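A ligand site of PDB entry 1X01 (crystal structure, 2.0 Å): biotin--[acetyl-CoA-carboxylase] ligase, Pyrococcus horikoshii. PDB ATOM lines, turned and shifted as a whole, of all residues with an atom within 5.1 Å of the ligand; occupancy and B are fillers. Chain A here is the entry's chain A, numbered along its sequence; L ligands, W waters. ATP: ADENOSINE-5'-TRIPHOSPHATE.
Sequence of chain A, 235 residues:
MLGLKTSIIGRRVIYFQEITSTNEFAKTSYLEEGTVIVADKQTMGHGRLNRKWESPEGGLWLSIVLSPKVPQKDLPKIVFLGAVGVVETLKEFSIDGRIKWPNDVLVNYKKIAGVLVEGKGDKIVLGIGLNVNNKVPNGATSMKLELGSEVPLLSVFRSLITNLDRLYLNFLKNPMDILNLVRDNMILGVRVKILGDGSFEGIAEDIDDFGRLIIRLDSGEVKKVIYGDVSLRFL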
ATOM      1  N   GLY A  47      -2.624 -18.930  -5.627  1.00  0.00           N
ATOM      2  CA  GLY A  47      -1.684 -17.826  -5.676  1.00  0.00           C
ATOM      3  C   GLY A  47      -1.870 -16.874  -4.501  1.00  0.00           C
ATOM      4  O   GLY A  47      -2.660 -17.160  -3.596  1.00  0.00           O
ATOM      5  N   ARG A  48      -1.155 -15.763  -4.517  1.00  0.00           N
ATOM      6  CA  ARG A  48      -1.247 -14.782  -3.434  1.00  0.00           C
ATOM      7  C   ARG A  48      -2.669 -14.227  -3.295  1.00  0.00           C
ATOM      8  O   ARG A  48      -3.153 -13.999  -2.186  1.00  0.00           O
ATOM      9  CB  ARG A  48      -0.263 -13.626  -3.658  1.00  0.00           C
ATOM     10  CG  ARG A  48      -0.301 -12.573  -2.544  1.00  0.00           C
ATOM     11  CD  ARG A  48       0.914 -11.657  -2.538  1.00  0.00           C
ATOM     12  NE  ARG A  48       0.908 -10.656  -3.595  1.00  0.00           N
ATOM     13  CZ  ARG A  48      -0.042  -9.745  -3.768  1.00  0.00           C
ATOM     14  NH1 ARG A  48      -1.091  -9.702  -2.963  1.00  0.00           N
ATOM     15  NH2 ARG A  48       0.055  -8.853  -4.750  1.00  0.00           N
ATOM     16  N   LEU A  49      -3.334 -14.023  -4.430  1.00  0.00           N
ATOM     17  CA  LEU A  49      -4.695 -13.511  -4.466  1.00  0.00           C
ATOM     18  C   LEU A  49      -5.703 -14.625  -4.180  1.00  0.00           C
ATOM     19  O   LEU A  49      -6.909 -14.442  -4.330  1.00  0.00           O
ATOM     20  CB  LEU A  49      -4.993 -12.900  -5.840  1.00  0.00           C
ATOM     21  CG  LEU A  49      -4.517 -11.482  -6.195  1.00  0.00           C
ATOM     22  CD1 LEU A  49      -3.342 -11.042  -5.339  1.00  0.00           C
ATOM     23  CD2 LEU A  49      -4.143 -11.453  -7.667  1.00  0.00           C
ATOM     24  N   ASN A  50      -5.191 -15.795  -3.765  1.00  0.00           N
ATOM     25  CA  ASN A  50      -6.040 -16.938  -3.451  1.00  0.00           C
ATOM     26  C   ASN A  50      -6.695 -17.498  -4.722  1.00  0.00           C
ATOM     27  O   ASN A  50      -7.749 -18.141  -4.660  1.00  0.00           O
ATOM     28  CB  ASN A  50      -7.117 -16.536  -2.438  1.00  0.00           C
ATOM     29  CG  ASN A  50      -7.812 -17.736  -1.818  1.00  0.00           C
ATOM     30  OD1 ASN A  50      -7.188 -18.565  -1.149  1.00  0.00           O
ATOM     31  ND2 ASN A  50      -9.111 -17.840  -2.046  1.00  0.00           N
ATOM     32  N   ARG A  51      -6.065 -17.244  -5.863  1.00  0.00           N
ATOM     33  CA  ARG A  51      -6.579 -17.720  -7.140  1.00  0.00           C
ATOM     34  C   ARG A  51      -5.911 -19.038  -7.513  1.00  0.00           C
ATOM     35  O   ARG A  51      -4.891 -19.397  -6.936  1.00  0.00           O
ATOM     36  CB  ARG A  51      -6.309 -16.663  -8.222  1.00  0.00           C
ATOM     37  CG  ARG A  51      -6.970 -15.325  -7.918  1.00  0.00           C
ATOM     38  CD  ARG A  51      -6.530 -14.230  -8.866  1.00  0.00           C
ATOM     39  NE  ARG A  51      -7.122 -12.943  -8.507  1.00  0.00           N
ATOM     40  CZ  ARG A  51      -6.809 -11.784  -9.079  1.00  0.00           C
ATOM     41  NH1 ARG A  51      -5.898 -11.744 -10.048  1.00  0.00           N
ATOM     42  NH2 ARG A  51      -7.398 -10.664  -8.675  1.00  0.00           N
ATOM     43  N   LYS A  52      -6.501 -19.751  -8.467  1.00  0.00           N
ATOM     44  CA  LYS A  52      -5.955 -21.040  -8.894  1.00  0.00           C
ATOM     45  C   LYS A  52      -4.600 -20.893  -9.577  1.00  0.00           C
ATOM     46  O   LYS A  52      -4.426 -20.051 -10.454  1.00  0.00           O
ATOM     47  CB  LYS A  52      -6.947 -21.733  -9.851  1.00  0.00           C
ATOM     48  CG  LYS A  52      -6.623 -23.197 -10.137  1.00  0.00           C
ATOM     49  CD  LYS A  52      -6.717 -24.027  -8.860  1.00  0.00           C
ATOM     50  CE  LYS A  52      -6.490 -25.515  -9.126  1.00  0.00           C
ATOM     51  NZ  LYS A  52      -5.136 -25.789  -9.693  1.00  0.00           N
ATOM     52  N   TRP A  53      -3.647 -21.729  -9.171  1.00  0.00           N
ATOM     53  CA  TRP A  53      -2.309 -21.716  -9.749  1.00  0.00           C
ATOM     54  C   TRP A  53      -2.020 -23.095 -10.341  1.00  0.00           C
ATOM     55  O   TRP A  53      -2.044 -24.098  -9.637  1.00  0.00           O
ATOM     56  CB  TRP A  53      -1.258 -21.356  -8.700  1.00  0.00           C
ATOM     57  CG  TRP A  53       0.160 -21.453  -9.194  1.00  0.00           C
ATOM     58  CD1 TRP A  53       0.907 -22.588  -9.364  1.00  0.00           C
ATOM     59  CD2 TRP A  53       1.002 -20.370  -9.636  1.00  0.00           C
ATOM     60  NE1 TRP A  53       2.139 -22.289  -9.887  1.00  0.00           N
ATOM     61  CE2 TRP A  53       2.223 -20.938 -10.060  1.00  0.00           C
ATOM     62  CE3 TRP A  53       0.835 -18.984  -9.710  1.00  0.00           C
ATOM     63  CZ2 TRP A  53       3.283 -20.150 -10.558  1.00  0.00           C
ATOM     64  CZ3 TRP A  53       1.882 -18.201 -10.207  1.00  0.00           C
ATOM     65  CH2 TRP A  53       3.082 -18.791 -10.619  1.00  0.00           C
ATOM     66  N   GLU A  54      -1.760 -23.135 -11.648  1.00  0.00           N
ATOM     67  CA  GLU A  54      -1.473 -24.405 -12.318  1.00  0.00           C
ATOM     68  C   GLU A  54      -0.111 -24.937 -11.894  1.00  0.00           C
ATOM     69  O   GLU A  54       0.908 -24.234 -11.990  1.00  0.00           O
ATOM     70  CB  GLU A  54      -1.498 -24.222 -13.839  1.00  0.00           C
ATOM     71  CG  GLU A  54      -2.832 -23.744 -14.401  1.00  0.00           C
ATOM     72  CD  GLU A  54      -4.012 -24.573 -13.899  1.00  0.00           C
ATOM     73  OE1 GLU A  54      -3.965 -25.816 -14.022  1.00  0.00           O
ATOM     74  OE2 GLU A  54      -4.987 -23.966 -13.392  1.00  0.00           O
ATOM     75  N   TRP A  61       7.623 -26.809  -7.712  1.00  0.00           N
ATOM     76  CA  TRP A  61       6.629 -26.385  -6.732  1.00  0.00           C
ATOM     77  C   TRP A  61       7.131 -26.717  -5.323  1.00  0.00           C
ATOM     78  O   TRP A  61       7.184 -27.878  -4.922  1.00  0.00           O
ATOM     79  CB  TRP A  61       5.313 -27.117  -7.023  1.00  0.00           C
ATOM     80  CG  TRP A  61       5.067 -27.330  -8.492  1.00  0.00           C
ATOM     81  CD1 TRP A  61       4.932 -28.530  -9.139  1.00  0.00           C
ATOM     82  CD2 TRP A  61       4.922 -26.323  -9.503  1.00  0.00           C
ATOM     83  NE1 TRP A  61       4.703 -28.331 -10.489  1.00  0.00           N
ATOM     84  CE2 TRP A  61       4.692 -26.992 -10.734  1.00  0.00           C
ATOM     85  CE3 TRP A  61       4.956 -24.918  -9.486  1.00  0.00           C
ATOM     86  CZ2 TRP A  61       4.500 -26.299 -11.943  1.00  0.00           C
ATOM     87  CZ3 TRP A  61       4.765 -24.226 -10.695  1.00  0.00           C
ATOM     88  CH2 TRP A  61       4.533 -24.924 -11.903  1.00  0.00           C
ATOM     89  N   LYS A 100       8.202  -8.271 -10.613  1.00  0.00           N
ATOM     90  CA  LYS A 100       7.012  -7.441 -10.690  1.00  0.00           C
ATOM     91  C   LYS A 100       6.546  -7.346  -9.247  1.00  0.00           C
ATOM     92  O   LYS A 100       6.142  -8.347  -8.655  1.00  0.00           O
ATOM     93  CB  LYS A 100       5.936  -8.095 -11.550  1.00  0.00           C
ATOM     94  CG  LYS A 100       4.557  -7.475 -11.381  1.00  0.00           C
ATOM     95  CD  LYS A 100       3.536  -8.237 -12.204  1.00  0.00           C
ATOM     96  CE  LYS A 100       2.136  -8.090 -11.651  1.00  0.00           C
ATOM     97  NZ  LYS A 100       1.215  -9.058 -12.331  1.00  0.00           N
ATOM     98  N   ASN A 103       5.618  -9.804  -5.798  1.00  0.00           N
ATOM     99  CA  ASN A 103       5.835 -11.248  -5.589  1.00  0.00           C
ATOM    100  C   ASN A 103       6.057 -12.056  -6.876  1.00  0.00           C
ATOM    101  O   ASN A 103       6.177 -13.282  -6.858  1.00  0.00           O
ATOM    102  CB  ASN A 103       4.630 -11.794  -4.837  1.00  0.00           C
ATOM    103  CG  ASN A 103       3.392 -11.587  -5.669  1.00  0.00           C
ATOM    104  OD1 ASN A 103       3.252 -10.615  -6.397  1.00  0.00           O
ATOM    105  ND2 ASN A 103       2.464 -12.556  -5.557  1.00  0.00           N
ATOM    106  N   ASP A 104       6.089 -11.362  -8.029  1.00  0.00           N
ATOM    107  CA  ASP A 104       6.211 -12.098  -9.283  1.00  0.00           C
ATOM    108  C   ASP A 104       7.577 -11.904  -9.958  1.00  0.00           C
ATOM    109  O   ASP A 104       8.256 -10.898  -9.795  1.00  0.00           O
ATOM    110  CB  ASP A 104       5.105 -11.648 -10.231  1.00  0.00           C
ATOM    111  CG  ASP A 104       3.749 -12.030  -9.632  1.00  0.00           C
ATOM    112  OD1 ASP A 104       3.638 -13.143  -9.124  1.00  0.00           O
ATOM    113  OD2 ASP A 104       2.837 -11.200  -9.682  1.00  0.00           O
ATOM    114  N   LYS A 111       4.886 -14.011 -16.931  1.00  0.00           N
ATOM    115  CA  LYS A 111       5.058 -14.655 -15.638  1.00  0.00           C
ATOM    116  C   LYS A 111       5.745 -16.021 -15.696  1.00  0.00           C
ATOM    117  O   LYS A 111       5.238 -16.948 -16.326  1.00  0.00           O
ATOM    118  CB  LYS A 111       3.690 -14.791 -14.972  1.00  0.00           C
ATOM    119  CG  LYS A 111       3.686 -14.976 -13.449  1.00  0.00           C
ATOM    120  CD  LYS A 111       2.265 -14.782 -12.942  1.00  0.00           C
ATOM    121  CE  LYS A 111       2.149 -14.963 -11.449  1.00  0.00           C
ATOM    122  NZ  LYS A 111       0.797 -14.554 -10.971  1.00  0.00           N
ATOM    123  N   ASN A 131       7.953 -22.109 -13.227  1.00  0.00           N
ATOM    124  CA  ASN A 131       7.682 -22.878 -14.437  1.00  0.00           C
ATOM    125  C   ASN A 131       9.000 -23.252 -15.108  1.00  0.00           C
ATOM    126  O   ASN A 131       9.718 -22.385 -15.610  1.00  0.00           O
ATOM    127  CB  ASN A 131       6.840 -22.059 -15.433  1.00  0.00           C
ATOM    128  CG  ASN A 131       5.488 -21.682 -14.874  1.00  0.00           C
ATOM    129  OD1 ASN A 131       4.776 -22.505 -14.313  1.00  0.00           O
ATOM    130  ND2 ASN A 131       5.114 -20.411 -15.058  1.00  0.00           N
ATOM    131  N   ASN A 134       7.163 -27.436 -17.542  1.00  0.00           N
ATOM    132  CA  ASN A 134       5.724 -27.670 -17.579  1.00  0.00           C
ATOM    133  C   ASN A 134       5.016 -26.753 -18.561  1.00  0.00           C
ATOM    134  O   ASN A 134       5.544 -25.707 -18.941  1.00  0.00           O
ATOM    135  CB  ASN A 134       5.128 -27.438 -16.188  1.00  0.00           C
ATOM    136  CG  ASN A 134       5.491 -26.072 -15.641  1.00  0.00           C
ATOM    137  OD1 ASN A 134       6.651 -25.802 -15.327  1.00  0.00           O
ATOM    138  ND2 ASN A 134       4.494 -25.199 -15.520  1.00  0.00           N
ATOM    139  N   VAL A 136       2.322 -24.029 -19.573  1.00  0.00           N
ATOM    140  CA  VAL A 136       1.870 -22.887 -18.802  1.00  0.00           C
ATOM    141  C   VAL A 136       0.661 -22.219 -19.419  1.00  0.00           C
ATOM    142  O   VAL A 136       0.393 -22.367 -20.611  1.00  0.00           O
ATOM    143  CB  VAL A 136       2.995 -21.828 -18.670  1.00  0.00           C
ATOM    144  CG1 VAL A 136       4.235 -22.462 -18.050  1.00  0.00           C
ATOM    145  CG2 VAL A 136       3.323 -21.242 -20.044  1.00  0.00           C
ATOM    146  N   PRO A 137      -0.110 -21.480 -18.609  1.00  0.00           N
ATOM    147  CA  PRO A 137      -1.301 -20.795 -19.130  1.00  0.00           C
ATOM    148  C   PRO A 137      -0.880 -19.632 -20.025  1.00  0.00           C
ATOM    149  O   PRO A 137       0.260 -19.165 -19.951  1.00  0.00           O
ATOM    150  CB  PRO A 137      -2.022 -20.349 -17.870  1.00  0.00           C
ATOM    151  CG  PRO A 137      -0.895 -20.113 -16.906  1.00  0.00           C
ATOM    152  CD  PRO A 137      -0.003 -21.302 -17.146  1.00  0.00           C
ATOM    153  N   ALA A 140       1.900 -16.586 -19.496  1.00  0.00           N
ATOM    154  CA  ALA A 140       3.032 -17.032 -18.695  1.00  0.00           C
ATOM    155  C   ALA A 140       4.105 -17.598 -19.596  1.00  0.00           C
ATOM    156  O   ALA A 140       3.924 -17.681 -20.806  1.00  0.00           O
ATOM    157  CB  ALA A 140       2.574 -18.086 -17.722  1.00  0.00           C
ATOM    158  N   ARG A 233      -1.019  -3.807 -12.189  1.00  0.00           N
ATOM    159  CA  ARG A 233      -1.172  -4.071 -13.614  1.00  0.00           C
ATOM    160  C   ARG A 233      -0.328  -3.103 -14.436  1.00  0.00           C
ATOM    161  O   ARG A 233      -0.414  -1.892 -14.249  1.00  0.00           O
ATOM    162  CB  ARG A 233      -2.637  -3.908 -14.031  1.00  0.00           C
ATOM    163  CG  ARG A 233      -3.520  -5.096 -13.686  1.00  0.00           C
ATOM    164  CD  ARG A 233      -3.231  -6.294 -14.596  1.00  0.00           C
ATOM    165  NE  ARG A 233      -3.978  -7.472 -14.191  1.00  0.00           N
ATOM    166  CZ  ARG A 233      -5.311  -7.539 -14.139  1.00  0.00           C
ATOM    167  NH1 ARG A 233      -6.053  -6.491 -14.460  1.00  0.00           N
ATOM    168  NH2 ARG A 233      -5.899  -8.660 -13.740  1.00  0.00           N
HETATM  169  PG  ATP L   1      -1.563 -11.692 -11.214  1.00  0.00           P
HETATM  170  O1G ATP L   1      -1.682 -13.072 -11.826  1.00  0.00           O
HETATM  171  O2G ATP L   1      -2.700 -10.827 -11.740  1.00  0.00           O
HETATM  172  O3G ATP L   1      -0.222 -11.086 -11.576  1.00  0.00           O
HETATM  173  PB  ATP L   1      -0.719 -12.254  -8.452  1.00  0.00           P
HETATM  174  O1B ATP L   1      -0.977 -11.664  -7.111  1.00  0.00           O
HETATM  175  O2B ATP L   1       0.669 -11.922  -8.883  1.00  0.00           O
HETATM  176  O3B ATP L   1      -1.807 -11.728  -9.583  1.00  0.00           O
HETATM  177  PA  ATP L   1      -2.256 -14.661  -8.134  1.00  0.00           P
HETATM  178  O1A ATP L   1      -2.664 -14.577  -6.722  1.00  0.00           O
HETATM  179  O2A ATP L   1      -3.364 -14.204  -9.023  1.00  0.00           O
HETATM  180  O3A ATP L   1      -0.884 -13.840  -8.499  1.00  0.00           O
HETATM  181  O5' ATP L   1      -1.864 -16.176  -8.409  1.00  0.00           O
HETATM  182  C5' ATP L   1      -1.374 -16.623  -9.702  1.00  0.00           C
HETATM  183  C4' ATP L   1      -2.100 -16.158 -10.957  1.00  0.00           C
HETATM  184  O4' ATP L   1      -1.195 -16.540 -12.028  1.00  0.00           O
HETATM  185  C3' ATP L   1      -3.436 -16.861 -11.262  1.00  0.00           C
HETATM  186  O3' ATP L   1      -4.546 -16.035 -10.877  1.00  0.00           O
HETATM  187  C2' ATP L   1      -3.353 -17.159 -12.770  1.00  0.00           C
HETATM  188  O2' ATP L   1      -3.990 -16.147 -13.567  1.00  0.00           O
HETATM  189  C1' ATP L   1      -1.853 -17.173 -13.103  1.00  0.00           C
HETATM  190  N9  ATP L   1      -1.198 -18.500 -13.150  1.00  0.00           N
HETATM  191  C8  ATP L   1      -1.690 -19.755 -12.767  1.00  0.00           C
HETATM  192  N7  ATP L   1      -0.829 -20.743 -12.926  1.00  0.00           N
HETATM  193  C5  ATP L   1       0.297 -20.126 -13.430  1.00  0.00           C
HETATM  194  C6  ATP L   1       1.568 -20.629 -13.846  1.00  0.00           C
HETATM  195  N6  ATP L   1       1.912 -21.926 -13.744  1.00  0.00           N
HETATM  196  N1  ATP L   1       2.497 -19.733 -14.329  1.00  0.00           N
HETATM  197  C2  ATP L   1       2.156 -18.427 -14.422  1.00  0.00           C
HETATM  198  N3  ATP L   1       0.987 -17.841 -14.072  1.00  0.00           N
HETATM  199  C4  ATP L   1       0.084 -18.745 -13.601  1.00  0.00           C
HETATM  200  O   HOH W   1      -0.450 -13.676 -14.386  1.00  0.00           O
HETATM  201  O   HOH W   2       0.161 -15.852 -16.005  1.00  0.00           O
HETATM  202  O   HOH W   3      -1.688  -9.038 -13.855  1.00  0.00           O
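OD2 of Asp 104 is in salt-bridge range of NZ of Lys 100. The side-chain carboxylate (OD1) of Asp 104 is in salt-bridge range of the side-chain amino group (NZ) of Lys 111 (3.7 Å). The side-chain carboxylate (OD2) of Asp 104 sits close to the side-chain amide oxygen (OD1) of Asn 103 (3.4 Å). The side-chain amide nitrogen (ND2) of Asn 134 sits at hydrogen-bond distance from the side-chain amide oxygen (OD1) of Asn 131 (3.0 Å). NE of Arg 48 sits close to ND2 of Asn 103, at 3.1 Å.
Merely in contact with the ligand: Gly 47, Trp 53, Ala 140, Lys 52, Pro 137 and Asn 103. Hydrophobic or aromatic side chains that line the ligand: Leu 49, Trp 53, Pro 137 and Ala 140.
The side-chain carboxylate (OD2) of Asp 104 lies close to an oxygen (O2B) of the ligand. N of Leu 49 lies within hydrogen-bond range of O1A of the ligand, at 2.5 Å. An oxygen (O3G) of the ligand lies within salt-bridge range of the side-chain amino group (NZ) of Lys 100 (2.6 Å). The side-chain amide nitrogen of Asn 131 lies within hydrogen-bond range of a nitrogen (N1) of the ligand, 2.8 Å away. A nitrogen (N7) of the ligand sits at hydrogen-bond distance from the backbone NH (N) of Glu 54 (2.9 Å). A nitrogen (N6) of the ligand sits at hydrogen-bond distance from the backbone carbonyl oxygen of Glu 54 (3.1 Å). An oxygen (O1A) of the ligand is in hydrogen-bond range of the backbone NH (N) of Arg 48 (2.9 Å). O1B of the ligand lies within salt-bridge range of NH2 of Arg 48 (3.8 Å). The side-chain amino group (NZ) of Lys 111 lies within salt-bridge range of an oxygen (O1G) of the ligand, 3.0 Å away. O2A of the ligand lies within salt-bridge range of NH1 of Arg 51 (3.7 Å).
Water W3 lies within hydrogen-bond range of NE of Arg 233 (2.8 Å), O2G of the ligand (2.9 Å) and NZ of Lys 100 (3.3 Å).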
